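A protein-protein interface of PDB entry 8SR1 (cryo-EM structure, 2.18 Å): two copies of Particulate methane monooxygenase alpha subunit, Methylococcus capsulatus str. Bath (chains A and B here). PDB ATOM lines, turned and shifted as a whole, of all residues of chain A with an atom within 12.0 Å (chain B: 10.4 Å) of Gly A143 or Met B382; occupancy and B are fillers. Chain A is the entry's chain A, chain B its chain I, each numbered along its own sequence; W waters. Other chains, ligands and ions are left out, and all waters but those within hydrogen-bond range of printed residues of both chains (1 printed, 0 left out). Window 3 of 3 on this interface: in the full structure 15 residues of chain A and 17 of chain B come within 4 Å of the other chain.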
ATOM      1  N   PRO A 137      24.662   4.777  27.528  1.00  0.00           N
ATOM      2  CA  PRO A 137      24.346   4.168  26.233  1.00  0.00           C
ATOM      3  C   PRO A 137      25.400   3.154  25.823  1.00  0.00           C
ATOM      4  O   PRO A 137      26.572   3.255  26.193  1.00  0.00           O
ATOM      5  CB  PRO A 137      24.327   5.365  25.276  1.00  0.00           C
ATOM      6  CG  PRO A 137      25.260   6.338  25.892  1.00  0.00           C
ATOM      7  CD  PRO A 137      25.129   6.167  27.382  1.00  0.00           C
ATOM      8  N   VAL A 138      24.964   2.163  25.052  1.00  0.00           N
ATOM      9  CA  VAL A 138      25.868   1.170  24.482  1.00  0.00           C
ATOM     10  C   VAL A 138      25.254   0.661  23.187  1.00  0.00           C
ATOM     11  O   VAL A 138      24.029   0.549  23.072  1.00  0.00           O
ATOM     12  CB  VAL A 138      26.155   0.017  25.469  1.00  0.00           C
ATOM     13  CG1 VAL A 138      24.931  -0.860  25.664  1.00  0.00           C
ATOM     14  CG2 VAL A 138      27.342  -0.802  24.995  1.00  0.00           C
ATOM     15  N   THR A 139      26.100   0.386  22.201  1.00  0.00           N
ATOM     16  CA  THR A 139      25.644  -0.118  20.914  1.00  0.00           C
ATOM     17  C   THR A 139      26.060  -1.574  20.761  1.00  0.00           C
ATOM     18  O   THR A 139      27.239  -1.911  20.911  1.00  0.00           O
ATOM     19  CB  THR A 139      26.216   0.719  19.770  1.00  0.00           C
ATOM     20  OG1 THR A 139      25.830   2.088  19.938  1.00  0.00           O
ATOM     21  CG2 THR A 139      25.705   0.212  18.430  1.00  0.00           C
ATOM     22  N   THR A 140      25.095  -2.430  20.457  1.00  0.00           N
ATOM     23  CA  THR A 140      25.345  -3.853  20.325  1.00  0.00           C
ATOM     24  C   THR A 140      25.780  -4.191  18.903  1.00  0.00           C
ATOM     25  O   THR A 140      25.666  -3.385  17.978  1.00  0.00           O
ATOM     26  CB  THR A 140      24.096  -4.654  20.698  1.00  0.00           C
ATOM     27  OG1 THR A 140      23.149  -4.583  19.629  1.00  0.00           O
ATOM     28  CG2 THR A 140      23.464  -4.089  21.960  1.00  0.00           C
ATOM     29  N   LEU A 141      26.294  -5.410  18.736  1.00  0.00           N
ATOM     30  CA  LEU A 141      26.658  -5.889  17.410  1.00  0.00           C
ATOM     31  C   LEU A 141      25.444  -6.192  16.547  1.00  0.00           C
ATOM     32  O   LEU A 141      25.606  -6.445  15.348  1.00  0.00           O
ATOM     33  CB  LEU A 141      27.544  -7.129  17.524  1.00  0.00           C
ATOM     34  CG  LEU A 141      28.968  -6.862  18.009  1.00  0.00           C
ATOM     35  CD1 LEU A 141      29.632  -8.146  18.459  1.00  0.00           C
ATOM     36  CD2 LEU A 141      29.784  -6.191  16.917  1.00  0.00           C
ATOM     37  N   THR A 142      24.243  -6.173  17.121  1.00  0.00           N
ATOM     38  CA  THR A 142      23.018  -6.330  16.353  1.00  0.00           C
ATOM     39  C   THR A 142      22.469  -5.002  15.849  1.00  0.00           C
ATOM     40  O   THR A 142      21.390  -4.983  15.249  1.00  0.00           O
ATOM     41  CB  THR A 142      21.950  -7.037  17.192  1.00  0.00           C
ATOM     42  OG1 THR A 142      21.879  -6.427  18.484  1.00  0.00           O
ATOM     43  CG2 THR A 142      22.295  -8.506  17.351  1.00  0.00           C
ATOM     44  N   GLY A 143      23.177  -3.899  16.088  1.00  0.00           N
ATOM     45  CA  GLY A 143      22.791  -2.616  15.536  1.00  0.00           C
ATOM     46  C   GLY A 143      21.730  -1.857  16.297  1.00  0.00           C
ATOM     47  O   GLY A 143      20.973  -1.097  15.682  1.00  0.00           O
ATOM     48  N   GLN A 144      21.650  -2.026  17.613  1.00  0.00           N
ATOM     49  CA  GLN A 144      20.698  -1.277  18.419  1.00  0.00           C
ATOM     50  C   GLN A 144      21.426  -0.614  19.575  1.00  0.00           C
ATOM     51  O   GLN A 144      22.350  -1.192  20.153  1.00  0.00           O
ATOM     52  CB  GLN A 144      19.576  -2.177  18.950  1.00  0.00           C
ATOM     53  CG  GLN A 144      20.028  -3.555  19.388  1.00  0.00           C
ATOM     54  CD  GLN A 144      19.031  -4.632  19.015  1.00  0.00           C
ATOM     55  OE1 GLN A 144      18.353  -4.539  17.991  1.00  0.00           O
ATOM     56  NE2 GLN A 144      18.933  -5.664  19.845  1.00  0.00           N
ATOM     57  N   THR A 145      21.004   0.603  19.907  1.00  0.00           N
ATOM     58  CA  THR A 145      21.580   1.365  21.005  1.00  0.00           C
ATOM     59  C   THR A 145      20.610   1.345  22.178  1.00  0.00           C
ATOM     60  O   THR A 145      19.443   1.720  22.028  1.00  0.00           O
ATOM     61  CB  THR A 145      21.875   2.805  20.580  1.00  0.00           C
ATOM     62  OG1 THR A 145      22.868   2.806  19.548  1.00  0.00           O
ATOM     63  CG2 THR A 145      22.380   3.615  21.764  1.00  0.00           C
ATOM     64  N   VAL A 146      21.095   0.912  23.339  1.00  0.00           N
ATOM     65  CA  VAL A 146      20.270   0.802  24.532  1.00  0.00           C
ATOM     66  C   VAL A 146      20.941   1.556  25.669  1.00  0.00           C
ATOM     67  O   VAL A 146      22.157   1.772  25.665  1.00  0.00           O
ATOM     68  CB  VAL A 146      20.017  -0.672  24.929  1.00  0.00           C
ATOM     69  CG1 VAL A 146      19.579  -1.486  23.724  1.00  0.00           C
ATOM     70  CG2 VAL A 146      21.258  -1.280  25.559  1.00  0.00           C
ATOM     71  N   ASP A 147      20.132   1.971  26.638  1.00  0.00           N
ATOM     72  CA  ASP A 147      20.641   2.589  27.852  1.00  0.00           C
ATOM     73  C   ASP A 147      20.685   1.545  28.961  1.00  0.00           C
ATOM     74  O   ASP A 147      19.651   0.999  29.355  1.00  0.00           O
ATOM     75  CB  ASP A 147      19.765   3.772  28.267  1.00  0.00           C
ATOM     76  CG  ASP A 147      20.419   4.652  29.319  1.00  0.00           C
ATOM     77  OD1 ASP A 147      21.268   4.156  30.087  1.00  0.00           O
ATOM     78  OD2 ASP A 147      20.080   5.853  29.380  1.00  0.00           O
ATOM     79  N   TYR A 151      17.561  -0.690  30.427  1.00  0.00           N
ATOM     80  CA  TYR A 151      17.364  -1.738  29.435  1.00  0.00           C
ATOM     81  C   TYR A 151      16.951  -3.038  30.114  1.00  0.00           C
ATOM     82  O   TYR A 151      17.542  -3.434  31.125  1.00  0.00           O
ATOM     83  CB  TYR A 151      18.646  -1.935  28.629  1.00  0.00           C
ATOM     84  CG  TYR A 151      18.652  -3.141  27.722  1.00  0.00           C
ATOM     85  CD1 TYR A 151      17.960  -3.130  26.520  1.00  0.00           C
ATOM     86  CD2 TYR A 151      19.362  -4.284  28.058  1.00  0.00           C
ATOM     87  CE1 TYR A 151      17.967  -4.224  25.683  1.00  0.00           C
ATOM     88  CE2 TYR A 151      19.375  -5.386  27.228  1.00  0.00           C
ATOM     89  CZ  TYR A 151      18.677  -5.348  26.041  1.00  0.00           C
ATOM     90  OH  TYR A 151      18.687  -6.441  25.208  1.00  0.00           O
ATOM     91  N   TYR A 226      15.825 -11.539  19.774  1.00  0.00           N
ATOM     92  CA  TYR A 226      17.215 -11.741  20.168  1.00  0.00           C
ATOM     93  C   TYR A 226      17.749 -13.079  19.647  1.00  0.00           C
ATOM     94  O   TYR A 226      18.169 -13.932  20.433  1.00  0.00           O
ATOM     95  CB  TYR A 226      17.374 -11.660  21.681  1.00  0.00           C
ATOM     96  CG  TYR A 226      16.536 -10.598  22.345  1.00  0.00           C
ATOM     97  CD1 TYR A 226      16.865  -9.256  22.237  1.00  0.00           C
ATOM     98  CD2 TYR A 226      15.411 -10.940  23.083  1.00  0.00           C
ATOM     99  CE1 TYR A 226      16.099  -8.285  22.845  1.00  0.00           C
ATOM    100  CE2 TYR A 226      14.638  -9.976  23.690  1.00  0.00           C
ATOM    101  CZ  TYR A 226      14.988  -8.649  23.569  1.00  0.00           C
ATOM    102  OH  TYR A 226      14.221  -7.682  24.177  1.00  0.00           O
ATOM    103  N   PRO A 227      17.734 -13.299  18.328  1.00  0.00           N
ATOM    104  CA  PRO A 227      18.242 -14.576  17.805  1.00  0.00           C
ATOM    105  C   PRO A 227      19.738 -14.741  17.985  1.00  0.00           C
ATOM    106  O   PRO A 227      20.240 -15.867  17.882  1.00  0.00           O
ATOM    107  CB  PRO A 227      17.859 -14.527  16.322  1.00  0.00           C
ATOM    108  CG  PRO A 227      17.842 -13.079  16.000  1.00  0.00           C
ATOM    109  CD  PRO A 227      17.404 -12.356  17.243  1.00  0.00           C
ATOM    110  N   ILE A 228      20.464 -13.660  18.246  1.00  0.00           N
ATOM    111  CA  ILE A 228      21.910 -13.690  18.406  1.00  0.00           C
ATOM    112  C   ILE A 228      22.219 -13.405  19.868  1.00  0.00           C
ATOM    113  O   ILE A 228      22.007 -12.287  20.352  1.00  0.00           O
ATOM    114  CB  ILE A 228      22.605 -12.680  17.486  1.00  0.00           C
ATOM    115  CG1 ILE A 228      22.437 -13.090  16.020  1.00  0.00           C
ATOM    116  CG2 ILE A 228      24.065 -12.560  17.845  1.00  0.00           C
ATOM    117  CD1 ILE A 228      21.824 -12.015  15.159  1.00  0.00           C
ATOM    118  N   THR A 229      22.717 -14.414  20.575  1.00  0.00           N
ATOM    119  CA  THR A 229      23.139 -14.271  21.959  1.00  0.00           C
ATOM    120  C   THR A 229      24.480 -14.962  22.152  1.00  0.00           C
ATOM    121  O   THR A 229      24.816 -15.912  21.440  1.00  0.00           O
ATOM    122  CB  THR A 229      22.112 -14.856  22.949  1.00  0.00           C
ATOM    123  OG1 THR A 229      21.930 -16.253  22.687  1.00  0.00           O
ATOM    124  CG2 THR A 229      20.777 -14.137  22.843  1.00  0.00           C
ATOM    125  N   THR B 258      37.773 -10.167  12.994  1.00  0.00           N
ATOM    126  CA  THR B 258      36.353 -10.450  12.886  1.00  0.00           C
ATOM    127  C   THR B 258      36.122 -11.704  12.058  1.00  0.00           C
ATOM    128  O   THR B 258      36.940 -12.075  11.212  1.00  0.00           O
ATOM    129  CB  THR B 258      35.584  -9.276  12.255  1.00  0.00           C
ATOM    130  OG1 THR B 258      36.137  -8.970  10.970  1.00  0.00           O
ATOM    131  CG2 THR B 258      35.655  -8.042  13.143  1.00  0.00           C
ATOM    132  N   TYR B 259      34.994 -12.359  12.323  1.00  0.00           N
ATOM    133  CA  TYR B 259      34.540 -13.496  11.538  1.00  0.00           C
ATOM    134  C   TYR B 259      33.036 -13.387  11.356  1.00  0.00           C
ATOM    135  O   TYR B 259      32.317 -12.988  12.275  1.00  0.00           O
ATOM    136  CB  TYR B 259      34.907 -14.829  12.204  1.00  0.00           C
ATOM    137  CG  TYR B 259      34.174 -15.103  13.496  1.00  0.00           C
ATOM    138  CD1 TYR B 259      34.452 -14.374  14.639  1.00  0.00           C
ATOM    139  CD2 TYR B 259      33.202 -16.089  13.567  1.00  0.00           C
ATOM    140  CE1 TYR B 259      33.790 -14.621  15.820  1.00  0.00           C
ATOM    141  CE2 TYR B 259      32.532 -16.344  14.745  1.00  0.00           C
ATOM    142  CZ  TYR B 259      32.831 -15.604  15.867  1.00  0.00           C
ATOM    143  OH  TYR B 259      32.169 -15.848  17.048  1.00  0.00           O
ATOM    144  N   ARG B 260      32.565 -13.737  10.162  1.00  0.00           N
ATOM    145  CA  ARG B 260      31.148 -13.642   9.850  1.00  0.00           C
ATOM    146  C   ARG B 260      30.380 -14.809  10.453  1.00  0.00           C
ATOM    147  O   ARG B 260      30.841 -15.953  10.434  1.00  0.00           O
ATOM    148  CB  ARG B 260      30.939 -13.608   8.337  1.00  0.00           C
ATOM    149  CG  ARG B 260      31.586 -12.421   7.650  1.00  0.00           C
ATOM    150  CD  ARG B 260      30.614 -11.261   7.558  1.00  0.00           C
ATOM    151  NE  ARG B 260      29.233 -11.698   7.716  1.00  0.00           N
ATOM    152  CZ  ARG B 260      28.262 -10.948   8.220  1.00  0.00           C
ATOM    153  NH1 ARG B 260      28.489  -9.713   8.635  1.00  0.00           N
ATOM    154  NH2 ARG B 260      27.034 -11.452   8.310  1.00  0.00           N
ATOM    155  N   VAL B 261      29.204 -14.508  10.996  1.00  0.00           N
ATOM    156  CA  VAL B 261      28.299 -15.529  11.519  1.00  0.00           C
ATOM    157  C   VAL B 261      26.996 -15.475  10.729  1.00  0.00           C
ATOM    158  O   VAL B 261      26.243 -14.497  10.847  1.00  0.00           O
ATOM    159  CB  VAL B 261      28.040 -15.334  13.021  1.00  0.00           C
ATOM    160  CG1 VAL B 261      27.280 -16.523  13.581  1.00  0.00           C
ATOM    161  CG2 VAL B 261      29.347 -15.135  13.764  1.00  0.00           C
ATOM    162  N   PRO B 262      26.687 -16.489   9.908  1.00  0.00           N
ATOM    163  CA  PRO B 262      27.541 -17.648   9.646  1.00  0.00           C
ATOM    164  C   PRO B 262      28.576 -17.366   8.562  1.00  0.00           C
ATOM    165  O   PRO B 262      28.426 -16.408   7.803  1.00  0.00           O
ATOM    166  CB  PRO B 262      26.551 -18.727   9.181  1.00  0.00           C
ATOM    167  CG  PRO B 262      25.200 -18.034   9.051  1.00  0.00           C
ATOM    168  CD  PRO B 262      25.432 -16.563   9.142  1.00  0.00           C
ATOM    169  N   ILE B 348      31.618 -18.584  18.685  1.00  0.00           N
ATOM    170  CA  ILE B 348      30.515 -17.744  19.134  1.00  0.00           C
ATOM    171  C   ILE B 348      29.825 -18.356  20.348  1.00  0.00           C
ATOM    172  O   ILE B 348      29.214 -17.641  21.153  1.00  0.00           O
ATOM    173  CB  ILE B 348      29.529 -17.501  17.976  1.00  0.00           C
ATOM    174  CG1 ILE B 348      28.605 -16.323  18.292  1.00  0.00           C
ATOM    175  CG2 ILE B 348      28.732 -18.763  17.663  1.00  0.00           C
ATOM    176  CD1 ILE B 348      27.434 -16.204  17.349  1.00  0.00           C
ATOM    177  N   ILE B 378      35.935 -10.828  17.163  1.00  0.00           N
ATOM    178  CA  ILE B 378      34.624 -10.197  17.265  1.00  0.00           C
ATOM    179  C   ILE B 378      33.735 -10.750  16.159  1.00  0.00           C
ATOM    180  O   ILE B 378      34.054 -10.569  14.976  1.00  0.00           O
ATOM    181  CB  ILE B 378      34.726  -8.669  17.166  1.00  0.00           C
ATOM    182  CG1 ILE B 378      35.699  -8.132  18.219  1.00  0.00           C
ATOM    183  CG2 ILE B 378      33.356  -8.042  17.311  1.00  0.00           C
ATOM    184  CD1 ILE B 378      35.328  -8.490  19.637  1.00  0.00           C
ATOM    185  N   PRO B 379      32.626 -11.412  16.482  1.00  0.00           N
ATOM    186  CA  PRO B 379      31.702 -11.846  15.434  1.00  0.00           C
ATOM    187  C   PRO B 379      31.016 -10.667  14.766  1.00  0.00           C
ATOM    188  O   PRO B 379      30.793  -9.617  15.375  1.00  0.00           O
ATOM    189  CB  PRO B 379      30.697 -12.719  16.193  1.00  0.00           C
ATOM    190  CG  PRO B 379      30.712 -12.163  17.579  1.00  0.00           C
ATOM    191  CD  PRO B 379      32.136 -11.743  17.831  1.00  0.00           C
ATOM    192  N   SER B 380      30.685 -10.850  13.493  1.00  0.00           N
ATOM    193  CA  SER B 380      29.918  -9.876  12.728  1.00  0.00           C
ATOM    194  C   SER B 380      28.703 -10.576  12.144  1.00  0.00           C
ATOM    195  O   SER B 380      28.827 -11.660  11.568  1.00  0.00           O
ATOM    196  CB  SER B 380      30.760  -9.247  11.613  1.00  0.00           C
ATOM    197  OG  SER B 380      31.025 -10.182  10.585  1.00  0.00           O
ATOM    198  N   PHE B 381      27.531  -9.963  12.298  1.00  0.00           N
ATOM    199  CA  PHE B 381      26.277 -10.597  11.910  1.00  0.00           C
ATOM    200  C   PHE B 381      25.601  -9.908  10.737  1.00  0.00           C
ATOM    201  O   PHE B 381      24.988 -10.581   9.902  1.00  0.00           O
ATOM    202  CB  PHE B 381      25.335 -10.657  13.123  1.00  0.00           C
ATOM    203  CG  PHE B 381      25.990 -11.194  14.361  1.00  0.00           C
ATOM    204  CD1 PHE B 381      26.122 -12.560  14.551  1.00  0.00           C
ATOM    205  CD2 PHE B 381      26.484 -10.339  15.331  1.00  0.00           C
ATOM    206  CE1 PHE B 381      26.732 -13.060  15.686  1.00  0.00           C
ATOM    207  CE2 PHE B 381      27.093 -10.830  16.466  1.00  0.00           C
ATOM    208  CZ  PHE B 381      27.218 -12.192  16.644  1.00  0.00           C
ATOM    209  N   MET B 382      25.685  -8.584  10.647  1.00  0.00           N
ATOM    210  CA  MET B 382      25.147  -7.874   9.492  1.00  0.00           C
ATOM    211  C   MET B 382      26.273  -7.384   8.585  1.00  0.00           C
ATOM    212  O   MET B 382      27.452  -7.543   8.901  1.00  0.00           O
ATOM    213  CB  MET B 382      24.273  -6.694   9.923  1.00  0.00           C
ATOM    214  CG  MET B 382      23.389  -6.975  11.124  1.00  0.00           C
ATOM    215  SD  MET B 382      24.230  -6.647  12.680  1.00  0.00           S
ATOM    216  CE  MET B 382      24.458  -4.873  12.575  1.00  0.00           C
HETATM  217  O   HOH W   1      26.378 -17.951  21.063  1.00  0.00           O
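Leu A141 touches Ile B378 (CD1 to CG2, 3.9 Å).
Leu A141 touches Pro B379.
Phe B381 touches Leu A141.
CE of Met B382 touches C of Thr A142, 3.8 Å away.
CE of Met B382 touches N of Gly A143, 3.9 Å away.
Phe B381 touches Ile A228.
Water W1 lies within hydrogen-bond range of the backbone carbonyl oxygen of Thr A229 (2.6 Å) and the backbone carbonyl oxygen of Ile B348 (2.9 Å).
SD of Met B382 lies close to O of Leu A141 (3.0 Å).
Of the 16 printed residues of chain A, 4 touch a printed residue of chain B.
Along chain A the printed residues that touch a printed residue of chain B span positions 141 to 228.
Hydrophobic or aromatic side chains of chain B within 4 Å of the printed part of chain A: Ile B378, Phe B381 and Met B382.
Along chain B the printed residues that touch a printed residue of chain A span positions 378 to 382.
The side-chain hydroxyl (OG1) of Thr A140 lies within hydrogen-bond range of the side-chain hydroxyl (OG1) of Thr A142 (2.5 Å).
NE2 of Gln A144 sits at hydrogen-bond distance from OG1 of Thr A142 (3.3 Å).
N of Tyr B259 sits at hydrogen-bond distance from O of Ile B378 (3.3 Å).
The guanidinium group of Arg B260 is in hydrogen-bond range of the backbone carbonyl oxygen of Phe B381, 2.7 Å away.
The guanidinium group of Arg B260 is in hydrogen-bond range of the backbone carbonyl oxygen of Met B382.
No position is printed for both chains.
Of the printed residues of chain B, Leu A141 touches Ile B378 (3.9 Å), Pro B379 (3.6 Å), Phe B381 (3.9 Å) and Met B382 (3.0 Å).
Thr A142 touches just one residue of chain B: Met B382.
Gly A143 touches one residue of chain B.
No residue of chain B comes within 4 Å of Gln A144.
Of the printed residues of chain B, Ile A228 touches Phe B381 (3.4 Å).
No residue of chain A comes within 4 Å of Ser B380.
Of the printed residues of chain A, Phe B381 touches Leu A141 (3.9 Å) and Ile A228 (3.4 Å).
Of chain A, only Leu A141, Thr A142 and Gly A143 come within 4 Å of Met B382.
The nearest residue of chain A that does not touch Met B382 is Thr A140 (5.7 Å).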
